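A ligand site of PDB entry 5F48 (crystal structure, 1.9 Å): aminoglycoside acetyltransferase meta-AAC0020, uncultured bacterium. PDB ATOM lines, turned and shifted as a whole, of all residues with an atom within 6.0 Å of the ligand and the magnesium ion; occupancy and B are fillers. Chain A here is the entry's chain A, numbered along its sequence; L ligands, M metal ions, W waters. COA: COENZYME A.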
ATOM      1  N   VAL A  34     -36.145 -32.591 -12.275  1.00  0.00           N
ATOM      2  CA  VAL A  34     -34.700 -32.527 -12.444  1.00  0.00           C
ATOM      3  C   VAL A  34     -34.077 -33.920 -12.288  1.00  0.00           C
ATOM      4  O   VAL A  34     -33.136 -34.263 -13.010  1.00  0.00           O
ATOM      5  CB  VAL A  34     -34.042 -31.550 -11.417  1.00  0.00           C
ATOM      6  CG1 VAL A  34     -32.510 -31.602 -11.528  1.00  0.00           C
ATOM      7  CG2 VAL A  34     -34.533 -30.127 -11.649  1.00  0.00           C
ATOM      8  N   PHE A  35     -34.610 -34.722 -11.373  1.00  0.00           N
ATOM      9  CA  PHE A  35     -34.070 -36.074 -11.163  1.00  0.00           C
ATOM     10  C   PHE A  35     -34.635 -37.056 -12.178  1.00  0.00           C
ATOM     11  O   PHE A  35     -34.305 -38.228 -12.163  1.00  0.00           O
ATOM     12  CB  PHE A  35     -34.363 -36.566  -9.738  1.00  0.00           C
ATOM     13  CG  PHE A  35     -33.662 -35.763  -8.661  1.00  0.00           C
ATOM     14  CD1 PHE A  35     -32.364 -35.321  -8.837  1.00  0.00           C
ATOM     15  CD2 PHE A  35     -34.324 -35.452  -7.482  1.00  0.00           C
ATOM     16  CE1 PHE A  35     -31.731 -34.588  -7.846  1.00  0.00           C
ATOM     17  CE2 PHE A  35     -33.693 -34.708  -6.501  1.00  0.00           C
ATOM     18  CZ  PHE A  35     -32.405 -34.276  -6.676  1.00  0.00           C
ATOM     19  N   TYR A  90     -29.897 -33.893   2.121  1.00  0.00           N
ATOM     20  CA  TYR A  90     -30.369 -35.074   1.421  1.00  0.00           C
ATOM     21  C   TYR A  90     -30.473 -34.872  -0.082  1.00  0.00           C
ATOM     22  O   TYR A  90     -29.783 -35.512  -0.859  1.00  0.00           O
ATOM     23  CB  TYR A  90     -31.723 -35.494   1.970  1.00  0.00           C
ATOM     24  CG  TYR A  90     -32.124 -36.873   1.490  1.00  0.00           C
ATOM     25  CD1 TYR A  90     -31.535 -38.009   2.035  1.00  0.00           C
ATOM     26  CD2 TYR A  90     -33.051 -37.035   0.484  1.00  0.00           C
ATOM     27  CE1 TYR A  90     -31.875 -39.263   1.596  1.00  0.00           C
ATOM     28  CE2 TYR A  90     -33.412 -38.297   0.038  1.00  0.00           C
ATOM     29  CZ  TYR A  90     -32.816 -39.409   0.601  1.00  0.00           C
ATOM     30  OH  TYR A  90     -33.153 -40.684   0.180  1.00  0.00           O
ATOM     31  N   ASP A  91     -31.320 -33.946  -0.495  1.00  0.00           N
ATOM     32  CA  ASP A  91     -31.460 -33.645  -1.894  1.00  0.00           C
ATOM     33  C   ASP A  91     -31.047 -32.197  -2.175  1.00  0.00           C
ATOM     34  O   ASP A  91     -31.245 -31.318  -1.343  1.00  0.00           O
ATOM     35  CB  ASP A  91     -32.910 -33.852  -2.341  1.00  0.00           C
ATOM     36  CG  ASP A  91     -33.190 -35.263  -2.803  1.00  0.00           C
ATOM     37  OD1 ASP A  91     -32.306 -35.895  -3.421  1.00  0.00           O
ATOM     38  OD2 ASP A  91     -34.308 -35.752  -2.546  1.00  0.00           O
ATOM     39  N   LEU A  92     -30.481 -31.965  -3.346  1.00  0.00           N
ATOM     40  CA  LEU A  92     -30.259 -30.605  -3.839  1.00  0.00           C
ATOM     41  C   LEU A  92     -30.484 -30.603  -5.333  1.00  0.00           C
ATOM     42  O   LEU A  92     -29.991 -31.489  -6.019  1.00  0.00           O
ATOM     43  CB  LEU A  92     -28.848 -30.121  -3.507  1.00  0.00           C
ATOM     44  CG  LEU A  92     -28.343 -28.908  -4.284  1.00  0.00           C
ATOM     45  CD1 LEU A  92     -29.169 -27.670  -3.877  1.00  0.00           C
ATOM     46  CD2 LEU A  92     -26.852 -28.698  -4.022  1.00  0.00           C
ATOM     47  N   ALA A  93     -31.236 -29.630  -5.827  1.00  0.00           N
ATOM     48  CA  ALA A  93     -31.416 -29.515  -7.257  1.00  0.00           C
ATOM     49  C   ALA A  93     -31.735 -28.073  -7.662  1.00  0.00           C
ATOM     50  O   ALA A  93     -32.222 -27.285  -6.861  1.00  0.00           O
ATOM     51  CB  ALA A  93     -32.524 -30.442  -7.743  1.00  0.00           C
ATOM     52  N   VAL A  94     -31.443 -27.758  -8.911  1.00  0.00           N
ATOM     53  CA  VAL A  94     -31.732 -26.443  -9.467  1.00  0.00           C
ATOM     54  C   VAL A  94     -32.381 -26.671 -10.813  1.00  0.00           C
ATOM     55  O   VAL A  94     -32.006 -27.582 -11.545  1.00  0.00           O
ATOM     56  CB  VAL A  94     -30.453 -25.589  -9.605  1.00  0.00           C
ATOM     57  CG1 VAL A  94     -30.719 -24.335 -10.430  1.00  0.00           C
ATOM     58  CG2 VAL A  94     -29.914 -25.223  -8.228  1.00  0.00           C
ATOM     59  N   ASP A  95     -33.411 -25.870 -11.103  1.00  0.00           N
ATOM     60  CA  ASP A  95     -34.094 -25.892 -12.382  1.00  0.00           C
ATOM     61  C   ASP A  95     -33.100 -25.862 -13.543  1.00  0.00           C
ATOM     62  O   ASP A  95     -32.193 -25.038 -13.568  1.00  0.00           O
ATOM     63  CB  ASP A  95     -35.061 -24.707 -12.468  1.00  0.00           C
ATOM     64  CG  ASP A  95     -36.048 -24.830 -13.619  1.00  0.00           C
ATOM     65  OD1 ASP A  95     -35.610 -24.945 -14.767  1.00  0.00           O
ATOM     66  OD2 ASP A  95     -37.265 -24.805 -13.344  1.00  0.00           O
ATOM     67  N   TRP A  98     -32.073 -22.901 -15.106  1.00  0.00           N
ATOM     68  CA  TRP A  98     -31.430 -21.906 -14.269  1.00  0.00           C
ATOM     69  C   TRP A  98     -30.097 -22.352 -13.694  1.00  0.00           C
ATOM     70  O   TRP A  98     -29.540 -21.664 -12.837  1.00  0.00           O
ATOM     71  CB  TRP A  98     -32.363 -21.510 -13.111  1.00  0.00           C
ATOM     72  CG  TRP A  98     -33.557 -20.773 -13.621  1.00  0.00           C
ATOM     73  CD1 TRP A  98     -34.791 -21.279 -13.862  1.00  0.00           C
ATOM     74  CD2 TRP A  98     -33.592 -19.390 -14.009  1.00  0.00           C
ATOM     75  NE1 TRP A  98     -35.615 -20.292 -14.361  1.00  0.00           N
ATOM     76  CE2 TRP A  98     -34.900 -19.133 -14.461  1.00  0.00           C
ATOM     77  CE3 TRP A  98     -32.655 -18.362 -14.013  1.00  0.00           C
ATOM     78  CZ2 TRP A  98     -35.295 -17.872 -14.907  1.00  0.00           C
ATOM     79  CZ3 TRP A  98     -33.048 -17.111 -14.450  1.00  0.00           C
ATOM     80  CH2 TRP A  98     -34.359 -16.872 -14.900  1.00  0.00           C
ATOM     81  N   GLN A  99     -29.590 -23.479 -14.171  1.00  0.00           N
ATOM     82  CA  GLN A  99     -28.351 -24.025 -13.637  1.00  0.00           C
ATOM     83  C   GLN A  99     -27.140 -23.201 -14.082  1.00  0.00           C
ATOM     84  O   GLN A  99     -27.246 -22.420 -15.021  1.00  0.00           O
ATOM     85  CB  GLN A  99     -28.203 -25.487 -14.040  1.00  0.00           C
ATOM     86  CG  GLN A  99     -29.171 -26.425 -13.300  1.00  0.00           C
ATOM     87  CD  GLN A  99     -29.042 -27.879 -13.712  1.00  0.00           C
ATOM     88  OE1 GLN A  99     -28.243 -28.222 -14.592  1.00  0.00           O
ATOM     89  NE2 GLN A  99     -29.826 -28.742 -13.080  1.00  0.00           N
ATOM     90  N   ARG A 100     -26.016 -23.378 -13.402  1.00  0.00           N
ATOM     91  CA  ARG A 100     -24.798 -22.594 -13.662  1.00  0.00           C
ATOM     92  C   ARG A 100     -25.009 -21.089 -13.512  1.00  0.00           C
ATOM     93  O   ARG A 100     -24.494 -20.308 -14.303  1.00  0.00           O
ATOM     94  CB  ARG A 100     -24.248 -22.890 -15.063  1.00  0.00           C
ATOM     95  CG  ARG A 100     -23.302 -24.059 -15.145  1.00  0.00           C
ATOM     96  CD  ARG A 100     -21.905 -23.707 -14.637  1.00  0.00           C
ATOM     97  NE  ARG A 100     -20.886 -24.525 -15.290  1.00  0.00           N
ATOM     98  CZ  ARG A 100     -19.602 -24.532 -14.956  1.00  0.00           C
ATOM     99  NH1 ARG A 100     -19.157 -23.757 -13.974  1.00  0.00           N
ATOM    100  NH2 ARG A 100     -18.759 -25.309 -15.611  1.00  0.00           N
ATOM    101  N   GLN A 101     -25.765 -20.676 -12.497  1.00  0.00           N
ATOM    102  CA  GLN A 101     -25.951 -19.239 -12.242  1.00  0.00           C
ATOM    103  C   GLN A 101     -25.587 -18.889 -10.801  1.00  0.00           C
ATOM    104  O   GLN A 101     -25.783 -17.763 -10.364  1.00  0.00           O
ATOM    105  CB  GLN A 101     -27.395 -18.813 -12.519  1.00  0.00           C
ATOM    106  CG  GLN A 101     -27.905 -19.178 -13.888  1.00  0.00           C
ATOM    107  CD  GLN A 101     -27.253 -18.396 -14.994  1.00  0.00           C
ATOM    108  OE1 GLN A 101     -27.149 -17.167 -14.929  1.00  0.00           O
ATOM    109  NE2 GLN A 101     -26.797 -19.092 -16.026  1.00  0.00           N
ATOM    110  N   GLY A 102     -25.069 -19.871 -10.053  1.00  0.00           N
ATOM    111  CA  GLY A 102     -24.673 -19.644  -8.677  1.00  0.00           C
ATOM    112  C   GLY A 102     -25.758 -19.962  -7.663  1.00  0.00           C
ATOM    113  O   GLY A 102     -25.581 -19.717  -6.466  1.00  0.00           O
ATOM    114  N   ILE A 103     -26.860 -20.526  -8.132  1.00  0.00           N
ATOM    115  CA  ILE A 103     -27.988 -20.811  -7.240  1.00  0.00           C
ATOM    116  C   ILE A 103     -27.637 -21.925  -6.267  1.00  0.00           C
ATOM    117  O   ILE A 103     -27.792 -21.762  -5.061  1.00  0.00           O
ATOM    118  CB  ILE A 103     -29.256 -21.190  -8.017  1.00  0.00           C
ATOM    119  CG1 ILE A 103     -29.779 -19.980  -8.799  1.00  0.00           C
ATOM    120  CG2 ILE A 103     -30.337 -21.671  -7.057  1.00  0.00           C
ATOM    121  CD1 ILE A 103     -30.931 -20.287  -9.709  1.00  0.00           C
ATOM    122  N   GLY A 104     -27.140 -23.057  -6.794  1.00  0.00           N
ATOM    123  CA  GLY A 104     -26.738 -24.176  -5.960  1.00  0.00           C
ATOM    124  C   GLY A 104     -25.791 -23.709  -4.863  1.00  0.00           C
ATOM    125  O   GLY A 104     -25.983 -24.013  -3.696  1.00  0.00           O
ATOM    126  N   LYS A 105     -24.776 -22.950  -5.245  1.00  0.00           N
ATOM    127  CA  LYS A 105     -23.812 -22.423  -4.291  1.00  0.00           C
ATOM    128  C   LYS A 105     -24.479 -21.575  -3.229  1.00  0.00           C
ATOM    129  O   LYS A 105     -24.139 -21.655  -2.054  1.00  0.00           O
ATOM    130  CB  LYS A 105     -22.731 -21.612  -5.014  1.00  0.00           C
ATOM    131  CG  LYS A 105     -21.514 -21.296  -4.159  1.00  0.00           C
ATOM    132  CD  LYS A 105     -20.655 -20.169  -4.761  1.00  0.00           C
ATOM    133  CE  LYS A 105     -21.309 -18.793  -4.573  1.00  0.00           C
ATOM    134  NZ  LYS A 105     -20.426 -17.668  -5.023  1.00  0.00           N
ATOM    135  N   LYS A 106     -25.445 -20.747  -3.620  1.00  0.00           N
ATOM    136  CA  LYS A 106     -26.075 -19.866  -2.647  1.00  0.00           C
ATOM    137  C   LYS A 106     -26.895 -20.678  -1.652  1.00  0.00           C
ATOM    138  O   LYS A 106     -26.969 -20.356  -0.466  1.00  0.00           O
ATOM    139  CB  LYS A 106     -26.928 -18.804  -3.331  1.00  0.00           C
ATOM    140  CG  LYS A 106     -26.096 -17.642  -3.840  1.00  0.00           C
ATOM    141  CD  LYS A 106     -26.878 -16.694  -4.733  1.00  0.00           C
ATOM    142  CE  LYS A 106     -25.964 -15.606  -5.234  1.00  0.00           C
ATOM    143  NZ  LYS A 106     -24.669 -16.211  -5.683  1.00  0.00           N
ATOM    144  N   GLN A 126     -23.844 -35.977   0.079  1.00  0.00           N
ATOM    145  CA  GLN A 126     -23.249 -37.052  -0.710  1.00  0.00           C
ATOM    146  C   GLN A 126     -23.661 -37.014  -2.162  1.00  0.00           C
ATOM    147  O   GLN A 126     -24.713 -36.472  -2.507  1.00  0.00           O
ATOM    148  CB  GLN A 126     -23.623 -38.395  -0.092  1.00  0.00           C
ATOM    149  CG  GLN A 126     -23.250 -38.483   1.373  1.00  0.00           C
ATOM    150  CD  GLN A 126     -23.478 -39.860   1.947  1.00  0.00           C
ATOM    151  OE1 GLN A 126     -24.349 -40.591   1.495  1.00  0.00           O
ATOM    152  NE2 GLN A 126     -22.665 -40.236   2.942  1.00  0.00           N
ATOM    153  N   ALA A 127     -22.833 -37.589  -3.005  1.00  0.00           N
ATOM    154  CA  ALA A 127     -23.141 -37.698  -4.430  1.00  0.00           C
ATOM    155  C   ALA A 127     -22.725 -39.062  -4.949  1.00  0.00           C
ATOM    156  O   ALA A 127     -21.785 -39.636  -4.433  1.00  0.00           O
ATOM    157  CB  ALA A 127     -22.440 -36.579  -5.219  1.00  0.00           C
ATOM    158  N   ASP A 131     -22.001 -39.569 -10.684  1.00  0.00           N
ATOM    159  CA  ASP A 131     -22.574 -38.250 -10.962  1.00  0.00           C
ATOM    160  C   ASP A 131     -21.508 -37.154 -11.105  1.00  0.00           C
ATOM    161  O   ASP A 131     -21.337 -36.327 -10.217  1.00  0.00           O
ATOM    162  CB  ASP A 131     -23.572 -37.873  -9.862  1.00  0.00           C
ATOM    163  CG  ASP A 131     -24.476 -36.732 -10.260  1.00  0.00           C
ATOM    164  OD1 ASP A 131     -24.200 -36.062 -11.283  1.00  0.00           O
ATOM    165  OD2 ASP A 131     -25.475 -36.502  -9.531  1.00  0.00           O
ATOM    166  N   TYR A 133     -21.271 -34.304 -12.686  1.00  0.00           N
ATOM    167  CA  TYR A 133     -21.658 -32.904 -12.559  1.00  0.00           C
ATOM    168  C   TYR A 133     -21.887 -32.506 -11.084  1.00  0.00           C
ATOM    169  O   TYR A 133     -21.471 -31.435 -10.657  1.00  0.00           O
ATOM    170  CB  TYR A 133     -22.915 -32.632 -13.382  1.00  0.00           C
ATOM    171  CG  TYR A 133     -22.705 -32.798 -14.871  1.00  0.00           C
ATOM    172  CD1 TYR A 133     -21.542 -32.338 -15.487  1.00  0.00           C
ATOM    173  CD2 TYR A 133     -23.660 -33.413 -15.675  1.00  0.00           C
ATOM    174  CE1 TYR A 133     -21.347 -32.466 -16.861  1.00  0.00           C
ATOM    175  CE2 TYR A 133     -23.468 -33.558 -17.046  1.00  0.00           C
ATOM    176  CZ  TYR A 133     -22.309 -33.081 -17.629  1.00  0.00           C
ATOM    177  OH  TYR A 133     -22.096 -33.216 -18.979  1.00  0.00           O
ATOM    178  N   ALA A 134     -22.509 -33.382 -10.313  1.00  0.00           N
ATOM    179  CA  ALA A 134     -22.680 -33.160  -8.873  1.00  0.00           C
ATOM    180  C   ALA A 134     -21.338 -33.060  -8.158  1.00  0.00           C
ATOM    181  O   ALA A 134     -21.141 -32.201  -7.302  1.00  0.00           O
ATOM    182  CB  ALA A 134     -23.518 -34.275  -8.250  1.00  0.00           C
ATOM    183  N   ASP A 136     -18.375 -32.259  -9.359  1.00  0.00           N
ATOM    184  CA  ASP A 136     -17.739 -30.999  -9.692  1.00  0.00           C
ATOM    185  C   ASP A 136     -18.372 -29.880  -8.855  1.00  0.00           C
ATOM    186  O   ASP A 136     -17.673 -28.988  -8.379  1.00  0.00           O
ATOM    187  CB  ASP A 136     -17.861 -30.683 -11.178  1.00  0.00           C
ATOM    188  CG  ASP A 136     -16.649 -31.141 -11.961  1.00  0.00           C
ATOM    189  OD1 ASP A 136     -16.838 -31.623 -13.088  1.00  0.00           O
ATOM    190  OD2 ASP A 136     -15.506 -30.995 -11.450  1.00  0.00           O
ATOM    191  N   PHE A 137     -19.689 -29.943  -8.673  1.00  0.00           N
ATOM    192  CA  PHE A 137     -20.341 -28.874  -7.916  1.00  0.00           C
ATOM    193  C   PHE A 137     -19.903 -28.887  -6.458  1.00  0.00           C
ATOM    194  O   PHE A 137     -19.466 -27.859  -5.930  1.00  0.00           O
ATOM    195  CB  PHE A 137     -21.878 -28.976  -7.982  1.00  0.00           C
ATOM    196  CG  PHE A 137     -22.562 -28.088  -6.992  1.00  0.00           C
ATOM    197  CD1 PHE A 137     -22.647 -26.719  -7.209  1.00  0.00           C
ATOM    198  CD2 PHE A 137     -23.086 -28.619  -5.823  1.00  0.00           C
ATOM    199  CE1 PHE A 137     -23.261 -25.890  -6.291  1.00  0.00           C
ATOM    200  CE2 PHE A 137     -23.694 -27.795  -4.891  1.00  0.00           C
ATOM    201  CZ  PHE A 137     -23.796 -26.430  -5.122  1.00  0.00           C
ATOM    202  N   TYR A 138     -20.013 -30.030  -5.785  1.00  0.00           N
ATOM    203  CA  TYR A 138     -19.683 -30.056  -4.360  1.00  0.00           C
ATOM    204  C   TYR A 138     -18.218 -29.708  -4.126  1.00  0.00           C
ATOM    205  O   TYR A 138     -17.869 -29.029  -3.157  1.00  0.00           O
ATOM    206  CB  TYR A 138     -20.020 -31.417  -3.737  1.00  0.00           C
ATOM    207  CG  TYR A 138     -21.508 -31.579  -3.570  1.00  0.00           C
ATOM    208  CD1 TYR A 138     -22.241 -30.663  -2.830  1.00  0.00           C
ATOM    209  CD2 TYR A 138     -22.189 -32.637  -4.185  1.00  0.00           C
ATOM    210  CE1 TYR A 138     -23.617 -30.791  -2.684  1.00  0.00           C
ATOM    211  CE2 TYR A 138     -23.575 -32.775  -4.038  1.00  0.00           C
ATOM    212  CZ  TYR A 138     -24.274 -31.851  -3.283  1.00  0.00           C
ATOM    213  OH  TYR A 138     -25.645 -31.975  -3.144  1.00  0.00           O
ATOM    214  N   SER A 140     -16.599 -27.577  -5.533  1.00  0.00           N
ATOM    215  CA  SER A 140     -16.367 -26.156  -5.705  1.00  0.00           C
ATOM    216  C   SER A 140     -16.883 -25.362  -4.520  1.00  0.00           C
ATOM    217  O   SER A 140     -16.813 -24.133  -4.507  1.00  0.00           O
ATOM    218  CB  SER A 140     -17.025 -25.662  -6.996  1.00  0.00           C
ATOM    219  OG  SER A 140     -18.417 -25.626  -6.803  1.00  0.00           O
HETATM  220  N1A COA L   1     -23.091 -28.280 -13.149  1.00  0.00           N
HETATM  221  C2A COA L   1     -23.145 -27.507 -12.065  1.00  0.00           C
HETATM  222  N3A COA L   1     -22.063 -26.983 -11.484  1.00  0.00           N
HETATM  223  C4A COA L   1     -20.841 -27.221 -11.999  1.00  0.00           C
HETATM  224  C5A COA L   1     -20.709 -28.031 -13.152  1.00  0.00           C
HETATM  225  C6A COA L   1     -21.917 -28.566 -13.738  1.00  0.00           C
HETATM  226  N6A COA L   1     -21.860 -29.380 -14.894  1.00  0.00           N
HETATM  227  N7A COA L   1     -19.373 -28.101 -13.457  1.00  0.00           N
HETATM  228  C8A COA L   1     -18.703 -27.373 -12.535  1.00  0.00           C
HETATM  229  N9A COA L   1     -19.579 -26.836 -11.653  1.00  0.00           N
HETATM  230  C1B COA L   1     -19.230 -25.996 -10.507  1.00  0.00           C
HETATM  231  C2B COA L   1     -18.625 -24.538 -11.044  1.00  0.00           C
HETATM  232  O2B COA L   1     -17.264 -24.397 -10.563  1.00  0.00           O
HETATM  233  C3B COA L   1     -19.415 -23.651 -10.589  1.00  0.00           C
HETATM  234  O3B COA L   1     -18.784 -22.298 -10.436  1.00  0.00           O
HETATM  235  P3B COA L   1     -18.518 -21.504 -11.779  1.00  0.00           P
HETATM  236  O7A COA L   1     -18.089 -20.086 -11.446  1.00  0.00           O
HETATM  237  O8A COA L   1     -17.455 -22.245 -12.549  1.00  0.00           O
HETATM  238  O9A COA L   1     -19.782 -21.449 -12.599  1.00  0.00           O
HETATM  239  C4B COA L   1     -19.984 -24.264  -9.267  1.00  0.00           C
HETATM  240  O4B COA L   1     -20.212 -25.747  -9.702  1.00  0.00           O
HETATM  241  C5B COA L   1     -21.115 -23.584  -8.821  1.00  0.00           C
HETATM  242  O5B COA L   1     -22.155 -23.792  -9.718  1.00  0.00           O
HETATM  243  P1A COA L   1     -23.628 -23.364  -9.424  1.00  0.00           P
HETATM  244  O1A COA L   1     -24.077 -22.424 -10.506  1.00  0.00           O
HETATM  245  O2A COA L   1     -23.828 -22.792  -8.067  1.00  0.00           O
HETATM  246  O3A COA L   1     -24.408 -24.683  -9.669  1.00  0.00           O
HETATM  247  P2A COA L   1     -25.913 -24.963  -9.858  1.00  0.00           P
HETATM  248  O4A COA L   1     -26.765 -23.802  -9.361  1.00  0.00           O
HETATM  249  O5A COA L   1     -26.238 -25.343 -11.286  1.00  0.00           O
HETATM  250  O6A COA L   1     -25.955 -26.261  -8.878  1.00  0.00           O
HETATM  251  CBP COA L   1     -26.877 -28.421  -8.962  1.00  0.00           C
HETATM  252  CCP COA L   1     -27.158 -26.963  -8.565  1.00  0.00           C
HETATM  253  CDP COA L   1     -27.564 -29.337  -7.938  1.00  0.00           C
HETATM  254  CEP COA L   1     -25.383 -28.692  -8.999  1.00  0.00           C
HETATM  255  CAP COA L   1     -27.471 -28.546 -10.349  1.00  0.00           C
HETATM  256  OAP COA L   1     -26.498 -28.592 -11.365  1.00  0.00           O
HETATM  257  C9P COA L   1     -28.433 -29.693 -10.465  1.00  0.00           C
HETATM  258  O9P COA L   1     -29.551 -29.589  -9.996  1.00  0.00           O
HETATM  259  N8P COA L   1     -28.018 -30.867 -11.155  1.00  0.00           N
HETATM  260  C7P COA L   1     -28.921 -32.009 -11.319  1.00  0.00           C
HETATM  261  C6P COA L   1     -29.331 -32.528  -9.952  1.00  0.00           C
HETATM  262  C5P COA L   1     -28.201 -32.967  -9.053  1.00  0.00           C
HETATM  263  O5P COA L   1     -27.300 -33.663  -9.517  1.00  0.00           O
HETATM  264  N4P COA L   1     -28.197 -32.544  -7.677  1.00  0.00           N
HETATM  265  C3P COA L   1     -27.128 -32.970  -6.776  1.00  0.00           C
HETATM  266  C2P COA L   1     -27.400 -34.443  -6.391  1.00  0.00           C
HETATM  267  S1P COA L   1     -28.845 -34.604  -5.305  1.00  0.00           S
HETATM  268 MG    MG M   1     -15.482 -22.581 -11.234  1.00  0.00          MG
HETATM  269  O   HOH W   1     -16.740 -19.500 -14.089  1.00  0.00           O
HETATM  270  O   HOH W   2     -25.471 -30.075 -13.887  1.00  0.00           O
HETATM  271  O   HOH W   3     -27.140 -34.847  -2.579  1.00  0.00           O
HETATM  272  O   HOH W   4     -22.058 -21.014 -11.117  1.00  0.00           O
HETATM  273  O   HOH W   5     -27.508 -21.699 -10.811  1.00  0.00           O
HETATM  274  O   HOH W   6     -18.673 -22.573  -7.231  1.00  0.00           O
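The side-chain carboxylate (OD2) of Asp 131 lies close to an oxygen (O5P) of the ligand, 3.4 Å away. CG1 of Val 34 touches C7P of the ligand (3.6 Å). Phe 35 touches the ligand. Ala 93 touches the ligand (CA to O9P, 3.3 Å). N of Ile 103 touches O4A of the ligand (3.5 Å). Tyr 133 touches the ligand (CD1 to N6A, 3.0 Å). Asp 136 touches the ligand. Phe 137 touches the ligand. Hydrophobic or aromatic side chains that line the ligand: Val 34, Phe 35, Leu 92, Ala 93, Val 94, Ile 103, Tyr 133 and Phe 137. Within 4 Å of the ligand: Val 34, Phe 35, Leu 92, Ala 93, Val 94, Gln 99, Arg 100, Gln 101, Gly 102, Ile 103, Gly 104, Lys 105, Asp 131, Tyr 133, Asp 136, Phe 137 and Ser 140. The nearest printed residue that does not touch the ligand is Ala 134 (4.04 Å).
NE2 of Gln 99 lies within hydrogen-bond range of O of Val 94 (2.9 Å). The side-chain hydroxyl (OG) of Ser 140 lies within hydrogen-bond range of the backbone carbonyl oxygen (O) of Phe 137 (2.6 Å). The backbone NH of Ala 134 sits at hydrogen-bond distance from the side-chain carboxylate of Asp 131 (3.3 Å).
No residue comes within 4 Å of the magnesium ion.
Water W4 lies within hydrogen-bond range of O1A of the ligand (2.5 Å) and N of Gly 102 (3.4 Å). Water W6 bridges OG of Ser 140 (3.1 Å) and O3B of the ligand (3.2 Å). Water W2 bridges N1A of the ligand (3.1 Å) and OE1 of Gln 99 (3.4 Å). Water W3 lies within hydrogen-bond range of O of Gln 126, O of Tyr 90, S1P of the ligand and OH of Tyr 138.
The magnesium ion is bound by O8A of the ligand. Slightly farther from the magnesium ion lies an oxygen (O2B) of the ligand (2.6 Å).
N of Leu 92 sits close to S1P of the ligand. O of Leu 92 lies within hydrogen-bond range of N4P of the ligand, 2.7 Å away. An oxygen (O4A) of the ligand sits at hydrogen-bond distance from the backbone NH (N) of Gly 104, 2.7 Å away. The guanidinium group (NH1) of Arg 100 lies within salt-bridge range of an oxygen (O9A) of the ligand (2.8 Å). The side-chain amide nitrogen (NE2) of Gln 99 sits close to an oxygen (O9P) of the ligand (3.2 Å). OG of Ser 140 sits close to O4B of the ligand. N of Gln 101 lies within hydrogen-bond range of O1A of the ligand (3.1 Å). O1A of the ligand sits at hydrogen-bond distance from N of Gly 102 (2.8 Å). The backbone NH (N) of Arg 100 sits at hydrogen-bond distance from an oxygen (O5A) of the ligand. An oxygen (O9P) of the ligand is in hydrogen-bond range of the backbone NH of Val 94. The backbone NH of Lys 105 sits at hydrogen-bond distance from an oxygen (O2A) of the ligand, 3.0 Å away.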
